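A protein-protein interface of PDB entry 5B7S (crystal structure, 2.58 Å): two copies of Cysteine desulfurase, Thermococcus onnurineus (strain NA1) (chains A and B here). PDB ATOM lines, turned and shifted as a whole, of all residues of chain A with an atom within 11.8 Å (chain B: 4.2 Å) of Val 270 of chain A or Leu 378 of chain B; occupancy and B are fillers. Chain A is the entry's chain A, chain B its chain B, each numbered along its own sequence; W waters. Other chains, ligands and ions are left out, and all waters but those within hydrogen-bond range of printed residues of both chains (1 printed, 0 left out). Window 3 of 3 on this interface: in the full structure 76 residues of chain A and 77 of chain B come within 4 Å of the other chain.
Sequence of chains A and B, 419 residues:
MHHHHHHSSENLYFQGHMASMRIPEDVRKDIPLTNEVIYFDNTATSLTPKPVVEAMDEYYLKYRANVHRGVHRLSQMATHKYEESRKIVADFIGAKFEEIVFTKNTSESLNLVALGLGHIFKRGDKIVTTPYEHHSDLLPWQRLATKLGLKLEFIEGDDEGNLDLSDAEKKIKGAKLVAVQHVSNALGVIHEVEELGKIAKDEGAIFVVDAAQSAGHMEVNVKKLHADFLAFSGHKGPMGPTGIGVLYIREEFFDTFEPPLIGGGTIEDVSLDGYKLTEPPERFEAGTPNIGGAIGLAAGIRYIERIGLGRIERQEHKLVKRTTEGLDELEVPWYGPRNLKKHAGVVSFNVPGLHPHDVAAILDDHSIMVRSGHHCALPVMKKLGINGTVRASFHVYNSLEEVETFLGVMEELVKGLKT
O of Asp 269 of chain A is in hydrogen-bond range of N of Lys 276 of chain A, 3.0 Å away. N of His 135 of chain B sits at hydrogen-bond distance from O of Cys 376 of chain B (2.7 Å). A ring nitrogen (NE2) of His 135 of chain B is in hydrogen-bond range of the backbone NH (N) of Leu 378 of chain B, 3.3 Å away.
Among the printed residues, pairs that only touch across the chains: Ile 262 of chain A with Leu 139 of chain B, Val 270 of chain A with His 135 of chain B, Gly 263 of chain A with Leu 139 of chain B, Ile 267 of chain A with His 135 of chain B, Ile 267 of chain A with Leu 139 of chain B, Tyr 275 of chain A with Leu 139 of chain B, Val 270 of chain A with Leu 378 of chain B, Gly 263 of chain A with His 135 of chain B, Ile 267 of chain A with His 374 of chain B, Asp 269 of chain A with Leu 378 of chain B and Gly 264 of chain A with His 135 of chain B.
Printed residues of chain B within 4 Å of Gly 263 of chain A: His 135 (3.96 Å) and Leu 139 (3.6 Å). Of the printed residues of chain B, Ile 267 of chain A touches His 135 (3.6 Å), Leu 139 (3.6 Å) and His 374 (3.98 Å). Val 270 of chain A touches two residues of chain B. Asp 273 of chain A touches none of the printed residues of chain B. His 374 of chain B touches one residue of chain A. No residue of chain A comes within 4 Å of Cys 376 of chain B. No residue of chain A comes within 4 Å of Ala 377 of chain B. Printed residues of chain A within 4 Å of Leu 378 of chain B: Asp 269 (3.99 Å) and Val 270 (3.7 Å). Pro 379 of chain B touches none of the printed residues of chain A. Val 380 of chain B touches none of the printed residues of chain A. No residue of chain A comes within 4 Å of Lys 382 of chain B. The nearest residue of chain B that does not touch Val 270 of chain A is Leu 139 of chain B (4.1 Å). The nearest printed residue of chain A that does not touch Leu 378 of chain B is Ile 267 of chain A (4.2 Å).
Of the 10 printed residues of chain B, 4 touch a printed residue of chain A. Hydrophobic or aromatic side chains of chain B that line the printed part of chain A: His 135, Leu 139, His 374 and Leu 378. Along chain A the printed residues that touch a printed residue of chain B span positions 262 to 275. Among the printed residues, 11 pairs touch across the chains.
No position is printed for both chains. Of the 11 pairs that touch across the chains among the printed residues, none has its exchanged pair printed and touching as well.
Water W1 lies within hydrogen-bond range of ND1 of His 135 of chain B, SG of Cys 376 of chain B and N of Gly 265 of chain A.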
ATOM      1  N   ILE A 262      15.882 -24.257  -6.139  1.00  0.00           N
ATOM      2  CA  ILE A 262      15.225 -24.111  -4.818  1.00  0.00           C
ATOM      3  C   ILE A 262      15.938 -23.082  -3.943  1.00  0.00           C
ATOM      4  O   ILE A 262      17.173 -22.915  -4.017  1.00  0.00           O
ATOM      5  CB  ILE A 262      15.177 -25.462  -4.052  1.00  0.00           C
ATOM      6  CG1 ILE A 262      16.539 -26.185  -4.124  1.00  0.00           C
ATOM      7  CG2 ILE A 262      14.090 -26.365  -4.622  1.00  0.00           C
ATOM      8  CD1 ILE A 262      16.666 -27.433  -3.265  1.00  0.00           C
ATOM      9  N   GLY A 263      15.148 -22.373  -3.138  1.00  0.00           N
ATOM     10  CA  GLY A 263      15.661 -21.482  -2.083  1.00  0.00           C
ATOM     11  C   GLY A 263      14.600 -20.495  -1.617  1.00  0.00           C
ATOM     12  O   GLY A 263      13.509 -20.899  -1.159  1.00  0.00           O
ATOM     13  N   GLY A 264      14.896 -19.203  -1.741  1.00  0.00           N
ATOM     14  CA  GLY A 264      13.944 -18.166  -1.324  1.00  0.00           C
ATOM     15  C   GLY A 264      12.584 -18.319  -1.989  1.00  0.00           C
ATOM     16  O   GLY A 264      12.520 -18.557  -3.198  1.00  0.00           O
ATOM     17  N   GLY A 265      11.511 -18.200  -1.197  1.00  0.00           N
ATOM     18  CA  GLY A 265      10.114 -18.393  -1.660  1.00  0.00           C
ATOM     19  C   GLY A 265       9.595 -19.821  -1.910  1.00  0.00           C
ATOM     20  O   GLY A 265       8.440 -20.007  -2.314  1.00  0.00           O
ATOM     21  N   THR A 266      10.423 -20.821  -1.610  1.00  0.00           N
ATOM     22  CA  THR A 266      10.246 -22.225  -2.041  1.00  0.00           C
ATOM     23  C   THR A 266       9.905 -23.196  -0.861  1.00  0.00           C
ATOM     24  O   THR A 266       9.765 -24.405  -1.059  1.00  0.00           O
ATOM     25  CB  THR A 266      11.539 -22.613  -2.849  1.00  0.00           C
ATOM     26  OG1 THR A 266      11.311 -22.461  -4.257  1.00  0.00           O
ATOM     27  CG2 THR A 266      12.082 -23.992  -2.591  1.00  0.00           C
ATOM     28  N   ILE A 267       9.688 -22.653   0.340  1.00  0.00           N
ATOM     29  CA  ILE A 267       9.772 -23.423   1.611  1.00  0.00           C
ATOM     30  C   ILE A 267       8.585 -23.215   2.570  1.00  0.00           C
ATOM     31  O   ILE A 267       7.933 -22.197   2.537  1.00  0.00           O
ATOM     32  CB  ILE A 267      11.100 -23.101   2.354  1.00  0.00           C
ATOM     33  CG1 ILE A 267      11.343 -21.574   2.527  1.00  0.00           C
ATOM     34  CG2 ILE A 267      12.269 -23.735   1.602  1.00  0.00           C
ATOM     35  CD1 ILE A 267      10.616 -20.883   3.679  1.00  0.00           C
ATOM     36  N   GLU A 268       8.302 -24.200   3.414  1.00  0.00           N
ATOM     37  CA  GLU A 268       7.397 -24.004   4.555  1.00  0.00           C
ATOM     38  C   GLU A 268       8.203 -23.766   5.823  1.00  0.00           C
ATOM     39  O   GLU A 268       7.858 -22.881   6.624  1.00  0.00           O
ATOM     40  CB  GLU A 268       6.423 -25.180   4.732  1.00  0.00           C
ATOM     41  CG  GLU A 268       5.102 -24.978   4.002  1.00  0.00           C
ATOM     42  CD  GLU A 268       4.087 -26.074   4.280  1.00  0.00           C
ATOM     43  OE1 GLU A 268       3.307 -26.409   3.356  1.00  0.00           O
ATOM     44  OE2 GLU A 268       4.056 -26.593   5.418  1.00  0.00           O
ATOM     45  N   ASP A 269       9.258 -24.568   6.009  1.00  0.00           N
ATOM     46  CA  ASP A 269      10.223 -24.359   7.098  1.00  0.00           C
ATOM     47  C   ASP A 269      11.628 -24.748   6.623  1.00  0.00           C
ATOM     48  O   ASP A 269      11.790 -25.481   5.646  1.00  0.00           O
ATOM     49  CB  ASP A 269       9.814 -25.138   8.380  1.00  0.00           C
ATOM     50  CG  ASP A 269      10.218 -24.416   9.675  1.00  0.00           C
ATOM     51  OD1 ASP A 269       9.473 -23.516  10.155  1.00  0.00           O
ATOM     52  OD2 ASP A 269      11.294 -24.748  10.208  1.00  0.00           O
ATOM     53  N   VAL A 270      12.633 -24.199   7.300  1.00  0.00           N
ATOM     54  CA  VAL A 270      14.042 -24.485   7.026  1.00  0.00           C
ATOM     55  C   VAL A 270      14.764 -24.389   8.358  1.00  0.00           C
ATOM     56  O   VAL A 270      14.365 -23.625   9.236  1.00  0.00           O
ATOM     57  CB  VAL A 270      14.699 -23.487   6.037  1.00  0.00           C
ATOM     58  CG1 VAL A 270      16.164 -23.844   5.768  1.00  0.00           C
ATOM     59  CG2 VAL A 270      13.951 -23.448   4.714  1.00  0.00           C
ATOM     60  N   SER A 271      15.808 -25.195   8.493  1.00  0.00           N
ATOM     61  CA  SER A 271      16.733 -25.125   9.607  1.00  0.00           C
ATOM     62  C   SER A 271      18.105 -25.522   9.062  1.00  0.00           C
ATOM     63  O   SER A 271      18.247 -25.792   7.871  1.00  0.00           O
ATOM     64  CB  SER A 271      16.287 -26.074  10.727  1.00  0.00           C
ATOM     65  OG  SER A 271      16.411 -27.426  10.315  1.00  0.00           O
ATOM     66  N   LEU A 272      19.098 -25.555   9.942  1.00  0.00           N
ATOM     67  CA  LEU A 272      20.453 -25.978   9.590  1.00  0.00           C
ATOM     68  C   LEU A 272      20.522 -27.481   9.251  1.00  0.00           C
ATOM     69  O   LEU A 272      21.395 -27.905   8.487  1.00  0.00           O
ATOM     70  CB  LEU A 272      21.423 -25.604  10.728  1.00  0.00           C
ATOM     71  CG  LEU A 272      21.572 -24.094  10.997  1.00  0.00           C
ATOM     72  CD1 LEU A 272      22.258 -23.798  12.324  1.00  0.00           C
ATOM     73  CD2 LEU A 272      22.318 -23.417   9.854  1.00  0.00           C
ATOM     74  N   ASP A 273      19.583 -28.263   9.804  1.00  0.00           N
ATOM     75  CA  ASP A 273      19.447 -29.703   9.510  1.00  0.00           C
ATOM     76  C   ASP A 273      18.963 -29.984   8.101  1.00  0.00           C
ATOM     77  O   ASP A 273      19.477 -30.876   7.444  1.00  0.00           O
ATOM     78  CB  ASP A 273      18.455 -30.374  10.470  1.00  0.00           C
ATOM     79  CG  ASP A 273      18.911 -30.321  11.910  1.00  0.00           C
ATOM     80  OD1 ASP A 273      19.111 -29.194  12.425  1.00  0.00           O
ATOM     81  OD2 ASP A 273      19.059 -31.406  12.522  1.00  0.00           O
ATOM     82  N   GLY A 274      17.947 -29.251   7.658  1.00  0.00           N
ATOM     83  CA  GLY A 274      17.287 -29.554   6.388  1.00  0.00           C
ATOM     84  C   GLY A 274      16.206 -28.571   6.005  1.00  0.00           C
ATOM     85  O   GLY A 274      16.116 -27.486   6.592  1.00  0.00           O
ATOM     86  N   TYR A 275      15.404 -28.956   5.008  1.00  0.00           N
ATOM     87  CA  TYR A 275      14.340 -28.114   4.455  1.00  0.00           C
ATOM     88  C   TYR A 275      13.042 -28.887   4.159  1.00  0.00           C
ATOM     89  O   TYR A 275      13.072 -30.042   3.732  1.00  0.00           O
ATOM     90  CB  TYR A 275      14.838 -27.374   3.198  1.00  0.00           C
ATOM     91  CG  TYR A 275      15.158 -28.243   1.993  1.00  0.00           C
ATOM     92  CD1 TYR A 275      14.147 -28.669   1.115  1.00  0.00           C
ATOM     93  CD2 TYR A 275      16.484 -28.604   1.692  1.00  0.00           C
ATOM     94  CE1 TYR A 275      14.445 -29.468   0.014  1.00  0.00           C
ATOM     95  CE2 TYR A 275      16.797 -29.391   0.581  1.00  0.00           C
ATOM     96  CZ  TYR A 275      15.780 -29.829  -0.251  1.00  0.00           C
ATOM     97  OH  TYR A 275      16.077 -30.613  -1.351  1.00  0.00           O
ATOM     98  N   LYS A 276      11.908 -28.234   4.413  1.00  0.00           N
ATOM     99  CA  LYS A 276      10.611 -28.677   3.924  1.00  0.00           C
ATOM    100  C   LYS A 276      10.133 -27.726   2.821  1.00  0.00           C
ATOM    101  O   LYS A 276      10.153 -26.515   3.019  1.00  0.00           O
ATOM    102  CB  LYS A 276       9.594 -28.712   5.056  1.00  0.00           C
ATOM    103  CG  LYS A 276       8.303 -29.415   4.643  1.00  0.00           C
ATOM    104  CD  LYS A 276       7.411 -29.733   5.833  1.00  0.00           C
ATOM    105  CE  LYS A 276       6.266 -30.662   5.453  1.00  0.00           C
ATOM    106  NZ  LYS A 276       5.266 -30.009   4.562  1.00  0.00           N
ATOM    107  N   LEU A 277       9.690 -28.264   1.679  1.00  0.00           N
ATOM    108  CA  LEU A 277       9.239 -27.445   0.540  1.00  0.00           C
ATOM    109  C   LEU A 277       7.763 -27.014   0.623  1.00  0.00           C
ATOM    110  O   LEU A 277       6.955 -27.668   1.275  1.00  0.00           O
ATOM    111  CB  LEU A 277       9.467 -28.195  -0.762  1.00  0.00           C
ATOM    112  CG  LEU A 277      10.909 -28.518  -1.121  1.00  0.00           C
ATOM    113  CD1 LEU A 277      10.914 -29.319  -2.416  1.00  0.00           C
ATOM    114  CD2 LEU A 277      11.747 -27.255  -1.266  1.00  0.00           C
ATOM    115  N   THR A 278       7.431 -25.922  -0.072  1.00  0.00           N
ATOM    116  CA  THR A 278       6.084 -25.338  -0.071  1.00  0.00           C
ATOM    117  C   THR A 278       5.187 -25.972  -1.146  1.00  0.00           C
ATOM    118  O   THR A 278       5.616 -26.888  -1.856  1.00  0.00           O
ATOM    119  CB  THR A 278       6.133 -23.771  -0.202  1.00  0.00           C
ATOM    120  OG1 THR A 278       4.856 -23.207   0.128  1.00  0.00           O
ATOM    121  CG2 THR A 278       6.532 -23.290  -1.605  1.00  0.00           C
ATOM    122  N   GLU A 282       4.720 -21.964  -6.249  1.00  0.00           N
ATOM    123  CA  GLU A 282       5.844 -21.263  -5.663  1.00  0.00           C
ATOM    124  C   GLU A 282       6.979 -22.221  -5.326  1.00  0.00           C
ATOM    125  O   GLU A 282       8.120 -21.807  -5.198  1.00  0.00           O
ATOM    126  CB  GLU A 282       5.410 -20.503  -4.395  1.00  0.00           C
ATOM    127  CG  GLU A 282       4.364 -19.380  -4.596  1.00  0.00           C
ATOM    128  CD  GLU A 282       2.912 -19.815  -4.376  1.00  0.00           C
ATOM    129  OE1 GLU A 282       2.657 -20.954  -3.904  1.00  0.00           O
ATOM    130  OE2 GLU A 282       2.004 -19.005  -4.674  1.00  0.00           O
ATOM    131  N   ARG A 283       6.679 -23.510  -5.170  1.00  0.00           N
ATOM    132  CA  ARG A 283       7.715 -24.494  -4.875  1.00  0.00           C
ATOM    133  C   ARG A 283       8.774 -24.565  -5.971  1.00  0.00           C
ATOM    134  O   ARG A 283       9.946 -24.808  -5.679  1.00  0.00           O
ATOM    135  CB  ARG A 283       7.126 -25.873  -4.542  1.00  0.00           C
ATOM    136  CG  ARG A 283       7.433 -26.995  -5.514  1.00  0.00           C
ATOM    137  CD  ARG A 283       7.459 -28.343  -4.823  1.00  0.00           C
ATOM    138  NE  ARG A 283       6.180 -28.676  -4.208  1.00  0.00           N
ATOM    139  CZ  ARG A 283       5.961 -29.777  -3.502  1.00  0.00           C
ATOM    140  NH1 ARG A 283       6.943 -30.664  -3.316  1.00  0.00           N
ATOM    141  NH2 ARG A 283       4.754 -29.996  -2.983  1.00  0.00           N
ATOM    142  N   HIS B 135      18.030 -18.412   2.461  1.00  0.00           N
ATOM    143  CA  HIS B 135      17.644 -19.777   2.044  1.00  0.00           C
ATOM    144  C   HIS B 135      18.293 -20.271   0.737  1.00  0.00           C
ATOM    145  O   HIS B 135      18.681 -21.432   0.634  1.00  0.00           O
ATOM    146  CB  HIS B 135      16.115 -19.935   1.996  1.00  0.00           C
ATOM    147  CG  HIS B 135      15.479 -19.912   3.352  1.00  0.00           C
ATOM    148  ND1 HIS B 135      14.158 -19.566   3.560  1.00  0.00           N
ATOM    149  CD2 HIS B 135      15.999 -20.165   4.575  1.00  0.00           C
ATOM    150  CE1 HIS B 135      13.892 -19.618   4.852  1.00  0.00           C
ATOM    151  NE2 HIS B 135      14.992 -19.985   5.489  1.00  0.00           N
ATOM    152  N   LEU B 139      20.057 -24.222   1.196  1.00  0.00           N
ATOM    153  CA  LEU B 139      19.350 -25.422   0.777  1.00  0.00           C
ATOM    154  C   LEU B 139      19.739 -26.005  -0.606  1.00  0.00           C
ATOM    155  O   LEU B 139      19.478 -27.170  -0.853  1.00  0.00           O
ATOM    156  CB  LEU B 139      17.846 -25.306   1.015  1.00  0.00           C
ATOM    157  CG  LEU B 139      17.009 -24.295   0.280  1.00  0.00           C
ATOM    158  CD1 LEU B 139      16.493 -24.927  -0.982  1.00  0.00           C
ATOM    159  CD2 LEU B 139      15.851 -23.842   1.158  1.00  0.00           C
ATOM    160  N   HIS B 374      10.388 -13.703   8.697  1.00  0.00           N
ATOM    161  CA  HIS B 374      11.653 -14.448   8.782  1.00  0.00           C
ATOM    162  C   HIS B 374      12.733 -14.061   7.722  1.00  0.00           C
ATOM    163  O   HIS B 374      13.882 -14.510   7.821  1.00  0.00           O
ATOM    164  CB  HIS B 374      11.392 -15.970   8.811  1.00  0.00           C
ATOM    165  CG  HIS B 374      10.770 -16.540   7.559  1.00  0.00           C
ATOM    166  ND1 HIS B 374       9.443 -16.919   7.486  1.00  0.00           N
ATOM    167  CD2 HIS B 374      11.312 -16.865   6.360  1.00  0.00           C
ATOM    168  CE1 HIS B 374       9.190 -17.419   6.289  1.00  0.00           C
ATOM    169  NE2 HIS B 374      10.310 -17.406   5.589  1.00  0.00           N
ATOM    170  N   CYS B 376      13.408 -14.872   4.596  1.00  0.00           N
ATOM    171  CA  CYS B 376      14.060 -16.017   3.939  1.00  0.00           C
ATOM    172  C   CYS B 376      15.366 -16.473   4.648  1.00  0.00           C
ATOM    173  O   CYS B 376      16.320 -16.911   3.989  1.00  0.00           O
ATOM    174  CB  CYS B 376      14.294 -15.719   2.430  1.00  0.00           C
ATOM    175  SG  CYS B 376      12.833 -15.338   1.390  1.00  0.00           S
ATOM    176  N   ALA B 377      15.388 -16.382   5.990  1.00  0.00           N
ATOM    177  CA  ALA B 377      16.560 -16.755   6.827  1.00  0.00           C
ATOM    178  C   ALA B 377      16.129 -17.270   8.221  1.00  0.00           C
ATOM    179  O   ALA B 377      16.648 -16.838   9.264  1.00  0.00           O
ATOM    180  CB  ALA B 377      17.512 -15.569   6.958  1.00  0.00           C
ATOM    181  N   LEU B 378      15.146 -18.173   8.213  1.00  0.00           N
ATOM    182  CA  LEU B 378      14.662 -18.862   9.402  1.00  0.00           C
ATOM    183  C   LEU B 378      15.750 -19.397  10.351  1.00  0.00           C
ATOM    184  O   LEU B 378      15.574 -19.312  11.558  1.00  0.00           O
ATOM    185  CB  LEU B 378      13.718 -20.012   9.011  1.00  0.00           C
ATOM    186  CG  LEU B 378      12.280 -19.630   8.640  1.00  0.00           C
ATOM    187  CD1 LEU B 378      11.607 -20.675   7.746  1.00  0.00           C
ATOM    188  CD2 LEU B 378      11.453 -19.385   9.899  1.00  0.00           C
ATOM    189  N   PRO B 379      16.857 -19.981   9.819  1.00  0.00           N
ATOM    190  CA  PRO B 379      17.946 -20.401  10.718  1.00  0.00           C
ATOM    191  C   PRO B 379      18.454 -19.296  11.634  1.00  0.00           C
ATOM    192  O   PRO B 379      18.679 -19.545  12.824  1.00  0.00           O
ATOM    193  CB  PRO B 379      19.036 -20.837   9.746  1.00  0.00           C
ATOM    194  CG  PRO B 379      18.270 -21.422   8.617  1.00  0.00           C
ATOM    195  CD  PRO B 379      17.067 -20.520   8.458  1.00  0.00           C
ATOM    196  N   VAL B 380      18.604 -18.091  11.073  1.00  0.00           N
ATOM    197  CA  VAL B 380      19.029 -16.904  11.825  1.00  0.00           C
ATOM    198  C   VAL B 380      18.043 -16.665  12.955  1.00  0.00           C
ATOM    199  O   VAL B 380      18.429 -16.672  14.119  1.00  0.00           O
ATOM    200  CB  VAL B 380      19.116 -15.637  10.945  1.00  0.00           C
ATOM    201  CG1 VAL B 380      19.496 -14.426  11.785  1.00  0.00           C
ATOM    202  CG2 VAL B 380      20.143 -15.802   9.840  1.00  0.00           C
ATOM    203  N   MET B 381      16.771 -16.516  12.593  1.00  0.00           N
ATOM    204  CA  MET B 381      15.647 -16.350  13.554  1.00  0.00           C
ATOM    205  C   MET B 381      15.654 -17.366  14.708  1.00  0.00           C
ATOM    206  O   MET B 381      15.331 -17.019  15.858  1.00  0.00           O
ATOM    207  CB  MET B 381      14.291 -16.471  12.839  1.00  0.00           C
ATOM    208  CG  MET B 381      14.024 -15.493  11.712  1.00  0.00           C
ATOM    209  SD  MET B 381      14.226 -13.785  12.232  1.00  0.00           S
ATOM    210  CE  MET B 381      15.943 -13.426  11.837  1.00  0.00           C
ATOM    211  N   LYS B 382      16.004 -18.611  14.368  1.00  0.00           N
ATOM    212  CA  LYS B 382      16.146 -19.711  15.324  1.00  0.00           C
ATOM    213  C   LYS B 382      17.380 -19.564  16.230  1.00  0.00           C
ATOM    214  O   LYS B 382      17.292 -19.818  17.434  1.00  0.00           O
ATOM    215  CB  LYS B 382      16.177 -21.052  14.582  1.00  0.00           C
HETATM  216  O   HOH W   1      12.009 -18.357   2.017  1.00  0.00           O
